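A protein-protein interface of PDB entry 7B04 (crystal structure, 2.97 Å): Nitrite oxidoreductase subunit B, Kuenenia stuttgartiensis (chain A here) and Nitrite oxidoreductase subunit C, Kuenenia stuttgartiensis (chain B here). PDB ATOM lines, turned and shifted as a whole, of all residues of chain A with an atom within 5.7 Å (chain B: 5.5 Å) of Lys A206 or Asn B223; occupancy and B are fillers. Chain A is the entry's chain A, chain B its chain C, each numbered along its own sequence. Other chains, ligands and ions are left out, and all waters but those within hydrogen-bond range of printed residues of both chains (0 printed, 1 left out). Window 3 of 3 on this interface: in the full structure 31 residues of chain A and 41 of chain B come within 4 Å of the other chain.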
ATOM      1  N   ASP A 204      16.263  -0.650  22.875  1.00  0.00           N
ATOM      2  CA  ASP A 204      15.438   0.445  23.377  1.00  0.00           C
ATOM      3  C   ASP A 204      16.352   1.498  23.988  1.00  0.00           C
ATOM      4  O   ASP A 204      16.934   1.282  25.057  1.00  0.00           O
ATOM      5  CB  ASP A 204      14.425  -0.073  24.396  1.00  0.00           C
ATOM      6  CG  ASP A 204      13.546   1.035  24.993  1.00  0.00           C
ATOM      7  OD1 ASP A 204      12.458   0.702  25.508  1.00  0.00           O
ATOM      8  OD2 ASP A 204      13.920   2.226  24.968  1.00  0.00           O
ATOM      9  N   GLN A 205      16.477   2.642  23.312  1.00  0.00           N
ATOM     10  CA  GLN A 205      17.352   3.702  23.797  1.00  0.00           C
ATOM     11  C   GLN A 205      16.775   4.422  25.010  1.00  0.00           C
ATOM     12  O   GLN A 205      17.528   5.076  25.739  1.00  0.00           O
ATOM     13  CB  GLN A 205      17.636   4.698  22.671  1.00  0.00           C
ATOM     14  CG  GLN A 205      18.433   4.098  21.525  1.00  0.00           C
ATOM     15  CD  GLN A 205      19.838   3.715  21.938  1.00  0.00           C
ATOM     16  OE1 GLN A 205      20.642   4.568  22.316  1.00  0.00           O
ATOM     17  NE2 GLN A 205      20.143   2.423  21.876  1.00  0.00           N
ATOM     18  N   LYS A 206      15.461   4.334  25.235  1.00  0.00           N
ATOM     19  CA  LYS A 206      14.873   4.904  26.442  1.00  0.00           C
ATOM     20  C   LYS A 206      15.165   4.060  27.679  1.00  0.00           C
ATOM     21  O   LYS A 206      15.310   4.608  28.777  1.00  0.00           O
ATOM     22  CB  LYS A 206      13.360   5.069  26.269  1.00  0.00           C
ATOM     23  CG  LYS A 206      12.663   5.703  27.467  1.00  0.00           C
ATOM     24  CD  LYS A 206      11.170   5.862  27.229  1.00  0.00           C
ATOM     25  CE  LYS A 206      10.478   6.453  28.448  1.00  0.00           C
ATOM     26  NZ  LYS A 206       9.018   6.641  28.227  1.00  0.00           N
ATOM     27  N   ARG A 207      15.282   2.739  27.523  1.00  0.00           N
ATOM     28  CA  ARG A 207      15.382   1.834  28.660  1.00  0.00           C
ATOM     29  C   ARG A 207      16.750   1.193  28.828  1.00  0.00           C
ATOM     30  O   ARG A 207      17.012   0.618  29.888  1.00  0.00           O
ATOM     31  CB  ARG A 207      14.343   0.709  28.541  1.00  0.00           C
ATOM     32  CG  ARG A 207      12.905   1.135  28.748  1.00  0.00           C
ATOM     33  CD  ARG A 207      11.980  -0.072  28.721  1.00  0.00           C
ATOM     34  NE  ARG A 207      12.204  -0.960  29.858  1.00  0.00           N
ATOM     35  CZ  ARG A 207      12.788  -2.151  29.776  1.00  0.00           C
ATOM     36  NH1 ARG A 207      12.948  -2.889  30.866  1.00  0.00           N
ATOM     37  NH2 ARG A 207      13.210  -2.607  28.604  1.00  0.00           N
ATOM     38  N   CYS A 208      17.621   1.273  27.824  1.00  0.00           N
ATOM     39  CA  CYS A 208      18.954   0.700  27.950  1.00  0.00           C
ATOM     40  C   CYS A 208      19.729   1.389  29.065  1.00  0.00           C
ATOM     41  O   CYS A 208      19.607   2.600  29.275  1.00  0.00           O
ATOM     42  CB  CYS A 208      19.709   0.826  26.628  1.00  0.00           C
ATOM     43  SG  CYS A 208      21.407   0.214  26.677  1.00  0.00           S
ATOM     44  N   ARG A 209      20.528   0.608  29.795  1.00  0.00           N
ATOM     45  CA  ARG A 209      21.317   1.138  30.900  1.00  0.00           C
ATOM     46  C   ARG A 209      22.813   0.889  30.729  1.00  0.00           C
ATOM     47  O   ARG A 209      23.566   0.966  31.706  1.00  0.00           O
ATOM     48  CB  ARG A 209      20.826   0.556  32.226  1.00  0.00           C
ATOM     49  CG  ARG A 209      19.451   1.062  32.641  1.00  0.00           C
ATOM     50  CD  ARG A 209      19.045   0.538  34.006  1.00  0.00           C
ATOM     51  NE  ARG A 209      19.903   1.050  35.071  1.00  0.00           N
ATOM     52  CZ  ARG A 209      19.716   2.210  35.691  1.00  0.00           C
ATOM     53  NH1 ARG A 209      20.547   2.590  36.652  1.00  0.00           N
ATOM     54  NH2 ARG A 209      18.700   2.992  35.352  1.00  0.00           N
ATOM     55  N   THR A 229      26.574   8.616  25.193  1.00  0.00           N
ATOM     56  CA  THR A 229      25.239   8.393  25.737  1.00  0.00           C
ATOM     57  C   THR A 229      25.218   7.388  26.879  1.00  0.00           C
ATOM     58  O   THR A 229      24.160   7.188  27.488  1.00  0.00           O
ATOM     59  CB  THR A 229      24.291   7.927  24.624  1.00  0.00           C
ATOM     60  OG1 THR A 229      24.848   6.783  23.964  1.00  0.00           O
ATOM     61  CG2 THR A 229      24.082   9.042  23.610  1.00  0.00           C
ATOM     62  N   VAL A 231      25.146   4.311  26.782  1.00  0.00           N
ATOM     63  CA  VAL A 231      24.301   3.177  26.432  1.00  0.00           C
ATOM     64  C   VAL A 231      24.814   2.604  25.116  1.00  0.00           C
ATOM     65  O   VAL A 231      25.573   3.244  24.386  1.00  0.00           O
ATOM     66  CB  VAL A 231      22.796   3.527  26.314  1.00  0.00           C
ATOM     67  CG1 VAL A 231      22.296   4.269  27.550  1.00  0.00           C
ATOM     68  CG2 VAL A 231      22.525   4.321  25.050  1.00  0.00           C
ATOM     69  N   GLY B 218      20.238   7.897  23.493  1.00  0.00           N
ATOM     70  CA  GLY B 218      19.811   8.363  24.814  1.00  0.00           C
ATOM     71  C   GLY B 218      19.611   9.849  24.797  1.00  0.00           C
ATOM     72  O   GLY B 218      18.692  10.318  25.434  1.00  0.00           O
ATOM     73  N   TYR B 219      20.455  10.577  24.085  1.00  0.00           N
ATOM     74  CA  TYR B 219      20.282  12.043  24.075  1.00  0.00           C
ATOM     75  C   TYR B 219      18.955  12.450  23.440  1.00  0.00           C
ATOM     76  O   TYR B 219      18.290  13.283  23.996  1.00  0.00           O
ATOM     77  CB  TYR B 219      21.469  12.723  23.407  1.00  0.00           C
ATOM     78  CG  TYR B 219      21.500  14.175  23.762  1.00  0.00           C
ATOM     79  CD1 TYR B 219      22.277  14.633  24.794  1.00  0.00           C
ATOM     80  CD2 TYR B 219      20.661  15.061  23.133  1.00  0.00           C
ATOM     81  CE1 TYR B 219      22.266  15.960  25.153  1.00  0.00           C
ATOM     82  CE2 TYR B 219      20.627  16.389  23.487  1.00  0.00           C
ATOM     83  CZ  TYR B 219      21.437  16.836  24.498  1.00  0.00           C
ATOM     84  OH  TYR B 219      21.415  18.146  24.837  1.00  0.00           O
ATOM     85  N   ALA B 221      16.316  10.453  23.003  1.00  0.00           N
ATOM     86  CA  ALA B 221      15.248   9.717  23.701  1.00  0.00           C
ATOM     87  C   ALA B 221      15.128  10.208  25.125  1.00  0.00           C
ATOM     88  O   ALA B 221      14.388   9.598  25.863  1.00  0.00           O
ATOM     89  CB  ALA B 221      15.514   8.247  23.678  1.00  0.00           C
ATOM     90  N   HIS B 222      15.949  11.183  25.490  1.00  0.00           N
ATOM     91  CA  HIS B 222      15.955  11.837  26.817  1.00  0.00           C
ATOM     92  C   HIS B 222      16.264  10.850  27.922  1.00  0.00           C
ATOM     93  O   HIS B 222      15.755  11.020  29.000  1.00  0.00           O
ATOM     94  CB  HIS B 222      14.694  12.653  27.017  1.00  0.00           C
ATOM     95  CG  HIS B 222      14.884  14.069  26.597  1.00  0.00           C
ATOM     96  ND1 HIS B 222      14.136  15.089  27.094  1.00  0.00           N
ATOM     97  CD2 HIS B 222      15.773  14.629  25.766  1.00  0.00           C
ATOM     98  CE1 HIS B 222      14.533  16.214  26.580  1.00  0.00           C
ATOM     99  NE2 HIS B 222      15.528  15.959  25.761  1.00  0.00           N
ATOM    100  N   ASN B 223      17.128   9.892  27.628  1.00  0.00           N
ATOM    101  CA  ASN B 223      17.554   8.896  28.624  1.00  0.00           C
ATOM    102  C   ASN B 223      18.402   9.672  29.612  1.00  0.00           C
ATOM    103  O   ASN B 223      19.200  10.450  29.177  1.00  0.00           O
ATOM    104  CB  ASN B 223      18.329   7.760  27.968  1.00  0.00           C
ATOM    105  CG  ASN B 223      18.952   6.815  28.957  1.00  0.00           C
ATOM    106  OD1 ASN B 223      19.519   7.237  29.945  1.00  0.00           O
ATOM    107  ND2 ASN B 223      18.865   5.536  28.684  1.00  0.00           N
ATOM    108  N   LEU B 224      18.228   9.411  30.891  1.00  0.00           N
ATOM    109  CA  LEU B 224      18.976  10.140  31.906  1.00  0.00           C
ATOM    110  C   LEU B 224      20.465   9.836  31.821  1.00  0.00           C
ATOM    111  O   LEU B 224      21.291  10.745  31.923  1.00  0.00           O
ATOM    112  CB  LEU B 224      18.430   9.810  33.292  1.00  0.00           C
ATOM    113  CG  LEU B 224      17.097  10.473  33.638  1.00  0.00           C
ATOM    114  CD1 LEU B 224      16.486   9.856  34.883  1.00  0.00           C
ATOM    115  CD2 LEU B 224      17.276  11.973  33.817  1.00  0.00           C
ATOM    116  N   LEU B 225      20.831   8.583  31.546  1.00  0.00           N
ATOM    117  CA  LEU B 225      22.251   8.245  31.486  1.00  0.00           C
ATOM    118  C   LEU B 225      22.991   9.007  30.392  1.00  0.00           C
ATOM    119  O   LEU B 225      24.227   9.043  30.405  1.00  0.00           O
ATOM    120  CB  LEU B 225      22.429   6.746  31.268  1.00  0.00           C
ATOM    121  CG  LEU B 225      21.748   5.818  32.267  1.00  0.00           C
ATOM    122  CD1 LEU B 225      22.101   4.387  31.952  1.00  0.00           C
ATOM    123  CD2 LEU B 225      22.168   6.163  33.683  1.00  0.00           C
ATOM    124  N   SER B 226      22.268   9.634  29.465  1.00  0.00           N
ATOM    125  CA  SER B 226      22.871  10.370  28.364  1.00  0.00           C
ATOM    126  C   SER B 226      22.806  11.882  28.538  1.00  0.00           C
ATOM    127  O   SER B 226      23.400  12.607  27.731  1.00  0.00           O
ATOM    128  CB  SER B 226      22.190   9.984  27.048  1.00  0.00           C
ATOM    129  OG  SER B 226      22.171   8.577  26.888  1.00  0.00           O
ATOM    130  N   LEU B 227      22.116  12.374  29.559  1.00  0.00           N
ATOM    131  CA  LEU B 227      21.897  13.797  29.756  1.00  0.00           C
ATOM    132  C   LEU B 227      22.669  14.324  30.961  1.00  0.00           C
ATOM    133  O   LEU B 227      23.151  13.551  31.794  1.00  0.00           O
ATOM    134  CB  LEU B 227      20.403  14.093  29.951  1.00  0.00           C
ATOM    135  CG  LEU B 227      19.450  13.780  28.798  1.00  0.00           C
ATOM    136  CD1 LEU B 227      18.020  14.093  29.204  1.00  0.00           C
ATOM    137  CD2 LEU B 227      19.838  14.562  27.554  1.00  0.00           C
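Hydrophobic or aromatic side chains of chain B that line the printed part of chain A: Leu B225.
Along chain B the printed residues that touch a printed residue of chain A span positions 218 to 226.
Along chain A the printed residues that touch a printed residue of chain B span positions 205 to 231.
Among the printed residues, no Asp or Glu carboxylate lies within 4 Å of a Lys or Arg side-chain nitrogen of the other chain.
Asp A204 touches none of the printed residues of chain B.
Printed residues of chain B within 4 Å of Lys A206: Asn B223.
Printed residues of chain A within 4 Å of Gly B218: Gln A205 (3.6 Å).
Of the printed residues of chain A, Tyr B219 touches Thr A229 (3.97 Å).
His B222 touches none of the printed residues of chain A.
Asn B223 touches just these residues of chain A: Gln A205 (3.3 Å), Lys A206 (3.7 Å), Cys A208 (3.1 Å) and Val A231 (3.8 Å).
Of the printed residues of chain A, Leu B225 touches Arg A209 (3.5 Å) and Thr A229 (3.5 Å).
The nearest residue of chain B that does not touch Lys A206 is Ala B221 (4.2 Å).
The nearest printed residue of chain A that does not touch Gly B218 is Thr A229 (4.01 Å).
ND2 of Asn B223 is in hydrogen-bond range of O of Gln A205, 3.3 Å away.
The backbone carbonyl oxygen of Cys A208 is in hydrogen-bond range of the side-chain amide nitrogen of Asn B223.
The side-chain hydroxyl (OG) of Ser B226 sits at hydrogen-bond distance from the backbone carbonyl oxygen (O) of Thr A229 (2.5 Å).
O of Leu B225 sits close to O of Thr A229.
The side-chain carboxylate (OD2) of Asp A204 is in hydrogen-bond range of the backbone NH (N) of Lys A206, at 2.6 Å.
The backbone carbonyl oxygen of Gly B218 sits at hydrogen-bond distance from the backbone NH of Asn B223, at 2.7 Å.
OD1 of Asn B223 lies within hydrogen-bond range of N of Leu B225, at 2.5 Å.
Among the printed residues, merely in contact across the chains: Gln A205 with Gly B218 (3.6 Å), Lys A206 with Asn B223 (3.7 Å), Arg A209 with Leu B225 (3.5 Å), Thr A229 with Tyr B219 (3.97 Å) and Val A231 with Asn B223 (3.8 Å).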
